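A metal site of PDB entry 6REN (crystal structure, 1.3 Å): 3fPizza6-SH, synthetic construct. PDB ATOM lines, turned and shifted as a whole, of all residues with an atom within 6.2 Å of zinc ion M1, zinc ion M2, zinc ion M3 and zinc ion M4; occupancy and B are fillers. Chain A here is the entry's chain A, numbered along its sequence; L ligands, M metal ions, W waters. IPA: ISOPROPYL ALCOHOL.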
ATOM      1  N   SER A  20      16.455 -29.294   8.814  1.00  0.00           N
ATOM      2  CA  SER A  20      17.320 -28.418   9.584  1.00  0.00           C
ATOM      3  C   SER A  20      18.180 -27.545   8.684  1.00  0.00           C
ATOM      4  O   SER A  20      17.850 -26.388   8.451  1.00  0.00           O
ATOM      5  CB  SER A  20      18.159 -29.227  10.592  1.00  0.00           C
ATOM      6  OG  SER A  20      19.006 -30.180   9.950  1.00  0.00           O
ATOM      7  N   GLY A  21      19.246 -28.073   8.145  1.00  0.00           N
ATOM      8  CA  GLY A  21      20.070 -27.277   7.269  1.00  0.00           C
ATOM      9  C   GLY A  21      19.449 -27.072   5.889  1.00  0.00           C
ATOM     10  O   GLY A  21      18.729 -27.932   5.364  1.00  0.00           O
ATOM     11  N   HIS A  35      16.864 -34.023   8.938  1.00  0.00           N
ATOM     12  CA  HIS A  35      17.634 -34.397  10.139  1.00  0.00           C
ATOM     13  C   HIS A  35      17.126 -35.684  10.763  1.00  0.00           C
ATOM     14  O   HIS A  35      17.932 -36.552  11.145  1.00  0.00           O
ATOM     15  CB  HIS A  35      17.497 -33.223  11.111  1.00  0.00           C
ATOM     16  CG  HIS A  35      18.389 -33.169  12.312  1.00  0.00           C
ATOM     17  ND1 HIS A  35      18.079 -33.754  13.531  1.00  0.00           N
ATOM     18  CD2 HIS A  35      19.482 -32.399  12.550  1.00  0.00           C
ATOM     19  CE1 HIS A  35      18.997 -33.423  14.424  1.00  0.00           C
ATOM     20  NE2 HIS A  35      19.865 -32.584  13.860  1.00  0.00           N
ATOM     21  N   THR A  60      21.694 -37.961  12.346  1.00  0.00           N
ATOM     22  CA  THR A  60      21.359 -36.561  12.578  1.00  0.00           C
ATOM     23  C   THR A  60      22.242 -35.595  11.775  1.00  0.00           C
ATOM     24  O   THR A  60      22.947 -34.751  12.335  1.00  0.00           O
ATOM     25  CB  THR A  60      21.279 -36.144  14.042  1.00  0.00           C
ATOM     26  OG1 THR A  60      22.467 -36.474  14.757  1.00  0.00           O
ATOM     27  CG2 THR A  60      20.099 -36.881  14.704  1.00  0.00           C
ATOM     28  N   PRO A  61      22.232 -35.703  10.447  1.00  0.00           N
ATOM     29  CA  PRO A  61      22.912 -34.689   9.616  1.00  0.00           C
ATOM     30  C   PRO A  61      22.263 -33.338   9.823  1.00  0.00           C
ATOM     31  O   PRO A  61      21.053 -33.219  10.016  1.00  0.00           O
ATOM     32  CB  PRO A  61      22.697 -35.201   8.186  1.00  0.00           C
ATOM     33  CG  PRO A  61      21.388 -35.953   8.278  1.00  0.00           C
ATOM     34  CD  PRO A  61      21.374 -36.607   9.640  1.00  0.00           C
ATOM     35  N   HIS A  62      23.068 -32.281   9.747  1.00  0.00           N
ATOM     36  CA  HIS A  62      22.581 -30.982  10.212  1.00  0.00           C
ATOM     37  C   HIS A  62      22.937 -29.892   9.192  1.00  0.00           C
ATOM     38  O   HIS A  62      22.144 -29.560   8.330  1.00  0.00           O
ATOM     39  CB  HIS A  62      23.089 -30.752  11.629  1.00  0.00           C
ATOM     40  CG  HIS A  62      22.419 -29.606  12.329  1.00  0.00           C
ATOM     41  ND1 HIS A  62      21.712 -29.768  13.504  1.00  0.00           N
ATOM     42  CD2 HIS A  62      22.347 -28.299  11.994  1.00  0.00           C
ATOM     43  CE1 HIS A  62      21.239 -28.574  13.883  1.00  0.00           C
ATOM     44  NE2 HIS A  62      21.604 -27.680  12.967  1.00  0.00           N
ATOM     45  N   GLY A  63      24.139 -29.363   9.185  1.00  0.00           N
ATOM     46  CA  GLY A  63      24.452 -28.326   8.211  1.00  0.00           C
ATOM     47  C   GLY A  63      24.699 -28.918   6.829  1.00  0.00           C
ATOM     48  O   GLY A  63      25.148 -30.074   6.683  1.00  0.00           O
ATOM     49  N   HIS A  77      26.539 -34.944  12.550  1.00  0.00           N
ATOM     50  CA  HIS A  77      27.017 -34.721  13.926  1.00  0.00           C
ATOM     51  C   HIS A  77      26.938 -35.937  14.819  1.00  0.00           C
ATOM     52  O   HIS A  77      27.762 -36.044  15.722  1.00  0.00           O
ATOM     53  CB  HIS A  77      26.586 -33.439  14.639  1.00  0.00           C
ATOM     54  CG  HIS A  77      25.118 -33.277  14.874  1.00  0.00           C
ATOM     55  ND1 HIS A  77      24.386 -34.073  15.742  1.00  0.00           N
ATOM     56  CD2 HIS A  77      24.257 -32.346  14.413  1.00  0.00           C
ATOM     57  CE1 HIS A  77      23.144 -33.630  15.791  1.00  0.00           C
ATOM     58  NE2 HIS A  77      23.034 -32.577  15.002  1.00  0.00           N
ATOM     59  N   SER A 104      27.953 -28.727  13.707  1.00  0.00           N
ATOM     60  CA  SER A 104      26.601 -28.325  13.311  1.00  0.00           C
ATOM     61  C   SER A 104      26.534 -27.665  11.963  1.00  0.00           C
ATOM     62  O   SER A 104      25.559 -27.876  11.248  1.00  0.00           O
ATOM     63  CB  SER A 104      25.961 -27.459  14.414  1.00  0.00           C
ATOM     64  OG  SER A 104      26.849 -26.411  14.732  1.00  0.00           O
ATOM     65  N   HIS A 119      30.551 -27.246  17.185  1.00  0.00           N
ATOM     66  CA  HIS A 119      29.607 -26.716  18.173  1.00  0.00           C
ATOM     67  C   HIS A 119      30.006 -27.108  19.606  1.00  0.00           C
ATOM     68  O   HIS A 119      30.055 -26.254  20.519  1.00  0.00           O
ATOM     69  CB  HIS A 119      28.249 -27.317  17.746  1.00  0.00           C
ATOM     70  CG  HIS A 119      27.019 -26.812  18.442  1.00  0.00           C
ATOM     71  ND1 HIS A 119      26.589 -27.274  19.662  1.00  0.00           N
ATOM     72  CD2 HIS A 119      26.015 -26.053  17.939  1.00  0.00           C
ATOM     73  CE1 HIS A 119      25.390 -26.768  19.920  1.00  0.00           C
ATOM     74  NE2 HIS A 119      25.021 -26.006  18.899  1.00  0.00           N
ATOM     75  N   THR A 144      29.231 -22.624  22.002  1.00  0.00           N
ATOM     76  CA  THR A 144      28.375 -23.380  21.091  1.00  0.00           C
ATOM     77  C   THR A 144      28.069 -22.626  19.790  1.00  0.00           C
ATOM     78  O   THR A 144      26.905 -22.339  19.487  1.00  0.00           O
ATOM     79  CB  THR A 144      27.098 -23.939  21.730  1.00  0.00           C
ATOM     80  OG1 THR A 144      26.244 -22.868  22.114  1.00  0.00           O
ATOM     81  CG2 THR A 144      27.387 -24.804  22.925  1.00  0.00           C
ATOM     82  N   PRO A 145      29.094 -22.299  19.019  1.00  0.00           N
ATOM     83  CA  PRO A 145      28.858 -21.721  17.683  1.00  0.00           C
ATOM     84  C   PRO A 145      28.124 -22.742  16.800  1.00  0.00           C
ATOM     85  O   PRO A 145      28.459 -23.930  16.791  1.00  0.00           O
ATOM     86  CB  PRO A 145      30.279 -21.448  17.167  1.00  0.00           C
ATOM     87  CG  PRO A 145      31.128 -22.547  17.857  1.00  0.00           C
ATOM     88  CD  PRO A 145      30.510 -22.677  19.243  1.00  0.00           C
ATOM     89  N   HIS A 146      27.129 -22.261  16.065  1.00  0.00           N
ATOM     90  CA  HIS A 146      26.121 -23.148  15.484  1.00  0.00           C
ATOM     91  C   HIS A 146      26.078 -23.044  13.965  1.00  0.00           C
ATOM     92  O   HIS A 146      26.444 -24.019  13.277  1.00  0.00           O
ATOM     93  CB  HIS A 146      24.770 -22.851  16.157  1.00  0.00           C
ATOM     94  CG  HIS A 146      23.651 -23.757  15.709  1.00  0.00           C
ATOM     95  ND1 HIS A 146      23.057 -24.696  16.523  1.00  0.00           N
ATOM     96  CD2 HIS A 146      23.062 -23.881  14.482  1.00  0.00           C
ATOM     97  CE1 HIS A 146      22.141 -25.341  15.830  1.00  0.00           C
ATOM     98  NE2 HIS A 146      22.112 -24.883  14.587  1.00  0.00           N
ATOM     99  N   GLY A 147      25.635 -21.916  13.417  1.00  0.00           N
ATOM    100  CA  GLY A 147      25.559 -21.704  11.984  1.00  0.00           C
ATOM    101  C   GLY A 147      26.815 -20.999  11.508  1.00  0.00           C
ATOM    102  O   GLY A 147      27.426 -20.229  12.255  1.00  0.00           O
ATOM    103  N   HIS A 161      25.595 -18.916  19.590  1.00  0.00           N
ATOM    104  CA  HIS A 161      24.352 -18.779  20.355  1.00  0.00           C
ATOM    105  C   HIS A 161      24.533 -18.964  21.852  1.00  0.00           C
ATOM    106  O   HIS A 161      23.671 -18.497  22.592  1.00  0.00           O
ATOM    107  CB  HIS A 161      23.152 -19.556  19.758  1.00  0.00           C
ATOM    108  CG  HIS A 161      23.225 -21.067  19.896  1.00  0.00           C
ATOM    109  ND1 HIS A 161      23.254 -21.747  21.103  1.00  0.00           N
ATOM    110  CD2 HIS A 161      23.159 -22.021  18.940  1.00  0.00           C
ATOM    111  CE1 HIS A 161      23.269 -23.060  20.870  1.00  0.00           C
ATOM    112  NE2 HIS A 161      23.211 -23.259  19.556  1.00  0.00           N
ATOM    113  N   PRO A 187      20.196 -17.581  18.217  1.00  0.00           N
ATOM    114  CA  PRO A 187      20.187 -17.717  16.750  1.00  0.00           C
ATOM    115  C   PRO A 187      20.750 -19.053  16.266  1.00  0.00           C
ATOM    116  O   PRO A 187      21.675 -19.613  16.871  1.00  0.00           O
ATOM    117  CB  PRO A 187      21.061 -16.554  16.286  1.00  0.00           C
ATOM    118  CG  PRO A 187      21.993 -16.306  17.433  1.00  0.00           C
ATOM    119  CD  PRO A 187      21.155 -16.550  18.673  1.00  0.00           C
ATOM    120  N   SER A 188      20.179 -19.539  15.150  1.00  0.00           N
ATOM    121  CA  SER A 188      20.604 -20.823  14.548  1.00  0.00           C
ATOM    122  C   SER A 188      21.203 -20.584  13.158  1.00  0.00           C
ATOM    123  O   SER A 188      22.415 -20.405  13.029  1.00  0.00           O
ATOM    124  CB  SER A 188      19.443 -21.837  14.549  1.00  0.00           C
ATOM    125  OG  SER A 188      18.244 -21.259  13.994  1.00  0.00           O
ATOM    126  N   GLY A 189      20.430 -20.623  12.085  1.00  0.00           N
ATOM    127  CA  GLY A 189      21.013 -20.452  10.760  1.00  0.00           C
ATOM    128  C   GLY A 189      21.488 -19.032  10.517  1.00  0.00           C
ATOM    129  O   GLY A 189      20.938 -18.050  11.036  1.00  0.00           O
ATOM    130  N   HIS A 203      15.949 -18.180  16.352  1.00  0.00           N
ATOM    131  CA  HIS A 203      15.186 -19.399  16.611  1.00  0.00           C
ATOM    132  C   HIS A 203      14.243 -19.248  17.789  1.00  0.00           C
ATOM    133  O   HIS A 203      13.106 -19.715  17.747  1.00  0.00           O
ATOM    134  CB  HIS A 203      16.190 -20.542  16.847  1.00  0.00           C
ATOM    135  CG  HIS A 203      15.625 -21.931  16.740  1.00  0.00           C
ATOM    136  ND1 HIS A 203      14.697 -22.471  17.621  1.00  0.00           N
ATOM    137  CD2 HIS A 203      15.926 -22.920  15.864  1.00  0.00           C
ATOM    138  CE1 HIS A 203      14.452 -23.736  17.272  1.00  0.00           C
ATOM    139  NE2 HIS A 203      15.215 -24.048  16.234  1.00  0.00           N
ATOM    140  N   THR A 228       8.408 -23.237  13.627  1.00  0.00           N
ATOM    141  CA  THR A 228       9.730 -23.308  14.269  1.00  0.00           C
ATOM    142  C   THR A 228      10.811 -23.246  13.186  1.00  0.00           C
ATOM    143  O   THR A 228      11.408 -24.269  12.813  1.00  0.00           O
ATOM    144  CB  THR A 228       9.849 -24.557  15.162  1.00  0.00           C
ATOM    145  OG1 THR A 228       8.718 -24.608  16.050  1.00  0.00           O
ATOM    146  CG2 THR A 228      11.108 -24.535  16.013  1.00  0.00           C
ATOM    147  N   PRO A 229      11.080 -22.076  12.638  1.00  0.00           N
ATOM    148  CA  PRO A 229      12.139 -21.952  11.618  1.00  0.00           C
ATOM    149  C   PRO A 229      13.512 -22.246  12.210  1.00  0.00           C
ATOM    150  O   PRO A 229      13.769 -22.054  13.412  1.00  0.00           O
ATOM    151  CB  PRO A 229      12.020 -20.488  11.177  1.00  0.00           C
ATOM    152  CG  PRO A 229      11.429 -19.767  12.383  1.00  0.00           C
ATOM    153  CD  PRO A 229      10.427 -20.776  12.920  1.00  0.00           C
ATOM    154  N   HIS A 230      14.430 -22.724  11.347  1.00  0.00           N
ATOM    155  CA  HIS A 230      15.728 -23.174  11.824  1.00  0.00           C
ATOM    156  C   HIS A 230      16.862 -22.739  10.907  1.00  0.00           C
ATOM    157  O   HIS A 230      17.738 -21.951  11.305  1.00  0.00           O
ATOM    158  CB  HIS A 230      15.733 -24.693  12.084  1.00  0.00           C
ATOM    159  CG  HIS A 230      17.003 -25.146  12.725  1.00  0.00           C
ATOM    160  ND1 HIS A 230      17.112 -25.540  14.036  1.00  0.00           N
ATOM    161  CD2 HIS A 230      18.258 -25.210  12.204  1.00  0.00           C
ATOM    162  CE1 HIS A 230      18.397 -25.785  14.310  1.00  0.00           C
ATOM    163  NE2 HIS A 230      19.127 -25.589  13.213  1.00  0.00           N
ATOM    164  N   GLY A 231      16.908 -23.275   9.695  1.00  0.00           N
ATOM    165  CA  GLY A 231      17.972 -22.946   8.760  1.00  0.00           C
ATOM    166  C   GLY A 231      17.540 -21.859   7.795  1.00  0.00           C
ATOM    167  O   GLY A 231      16.333 -21.683   7.518  1.00  0.00           O
ATOM    168  N   HIS A 245      11.015 -26.853  11.126  1.00  0.00           N
ATOM    169  CA  HIS A 245      10.806 -28.190  11.688  1.00  0.00           C
ATOM    170  C   HIS A 245       9.628 -28.257  12.640  1.00  0.00           C
ATOM    171  O   HIS A 245       9.346 -29.339  13.176  1.00  0.00           O
ATOM    172  CB  HIS A 245      12.085 -28.821  12.273  1.00  0.00           C
ATOM    173  CG  HIS A 245      12.750 -28.053  13.390  1.00  0.00           C
ATOM    174  ND1 HIS A 245      12.206 -27.930  14.646  1.00  0.00           N
ATOM    175  CD2 HIS A 245      13.941 -27.410  13.429  1.00  0.00           C
ATOM    176  CE1 HIS A 245      13.019 -27.221  15.402  1.00  0.00           C
ATOM    177  NE2 HIS A 245      14.093 -26.890  14.695  1.00  0.00           N
HETATM  178  C1  IPA L   1      14.798 -26.838  17.956  1.00  0.00           C
HETATM  179  C2  IPA L   1      16.256 -27.084  18.028  1.00  0.00           C
HETATM  180  C3  IPA L   1      16.776 -28.212  18.894  1.00  0.00           C
HETATM  181  O2  IPA L   1      16.741 -26.873  16.789  1.00  0.00           O
HETATM  182  C1  IPA L   2      22.568 -26.102  21.104  1.00  0.00           C
HETATM  183  C2  IPA L   2      21.625 -26.627  20.152  1.00  0.00           C
HETATM  184  C3  IPA L   2      20.434 -27.408  20.666  1.00  0.00           C
HETATM  185  O2  IPA L   2      21.683 -26.198  18.895  1.00  0.00           O
HETATM  186  C1  IPA L   3      19.716 -30.986  18.601  1.00  0.00           C
HETATM  187  C2  IPA L   3      19.953 -31.622  17.240  1.00  0.00           C
HETATM  188  C3  IPA L   3      20.481 -33.038  17.402  1.00  0.00           C
HETATM  189  O2  IPA L   3      20.709 -30.813  16.360  1.00  0.00           O
HETATM  190 ZN    ZN M   1      21.099 -25.711  13.049  1.00  0.00          ZN
HETATM  191 ZN    ZN M   2      15.672 -25.852  15.459  1.00  0.00          ZN
HETATM  192 ZN    ZN M   3      23.259 -25.016  18.542  1.00  0.00          ZN
HETATM  193 ZN    ZN M   4      21.391 -31.450  14.632  1.00  0.00          ZN
HETATM  194  O   HOH W   1      21.462 -24.430  11.119  1.00  0.00           O
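The nearest printed residue that does not touch zinc ion M1 is Ser 188 (4.5 Å).
Zinc ion M2 is bound by O2 of IPA L1 (2.0 Å), NE2 of His 203 (2.0 Å), NE2 of His 245 (2.0 Å) and ND1 of His 230 (2.0 Å).
Three residues have an atom within 4 Å of zinc ion M3: His 119, His 146 and His 161.
OG of Ser 188 lies within hydrogen-bond range of O of His 230, at 2.8 Å.
The backbone carbonyl oxygen (O) of His 230 sits at hydrogen-bond distance from the backbone NH (N) of Gly 189, 3.1 Å away.
ND1 of His 161 sits close to OG1 of Thr 144, 3.3 Å away.
The backbone carbonyl oxygen (O) of His 62 lies close to the backbone NH (N) of Gly 21, at 3.3 Å.
The backbone carbonyl oxygen (O) of His 146 is in hydrogen-bond range of the side-chain hydroxyl (OG) of Ser 104, 2.8 Å away.
N of His 245 is in hydrogen-bond range of O of Thr 228, 3.1 Å away.
ND1 of His 77 lies close to OG1 of Thr 60 (3.2 Å).
An oxygen (O2) of IPA L3 binds zinc ion M4, at 2.0 Å.
NE2 of His 77 binds zinc ion M4 (2.0 Å).
ND1 of His 62 is bound to zinc ion M4, at 2.1 Å.
Zinc ion M4 is bound by a ring nitrogen (NE2) of His 35 (2.1 Å).
Zinc ion M4 has four donor atoms within binding distance.
Of the 24 residues printed, 3 come within 4 Å of zinc ion M4.
The nearest printed residue that does not touch zinc ion M4 is Thr 60 (4.3 Å).
Of the 24 residues printed, 3 come within 4 Å of zinc ion M2.
The nearest printed residue that does not touch zinc ion M2 is Pro 229 (4.7 Å).
Zinc ion M3 is bound by an oxygen (O2) of IPA L2 (2.0 Å), a ring nitrogen (NE2) of His 161 (2.0 Å), a ring nitrogen (NE2) of His 119 (2.1 Å) and a ring nitrogen (ND1) of His 146 (2.1 Å).
Zinc ion M3 has four donor atoms within binding distance.
Zinc ion M1 is bound by a ring nitrogen (NE2) of His 230 (2.0 Å), a ring nitrogen (NE2) of His 146 (2.0 Å), a ring nitrogen (NE2) of His 62 (2.0 Å) and water W1 (2.3 Å).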
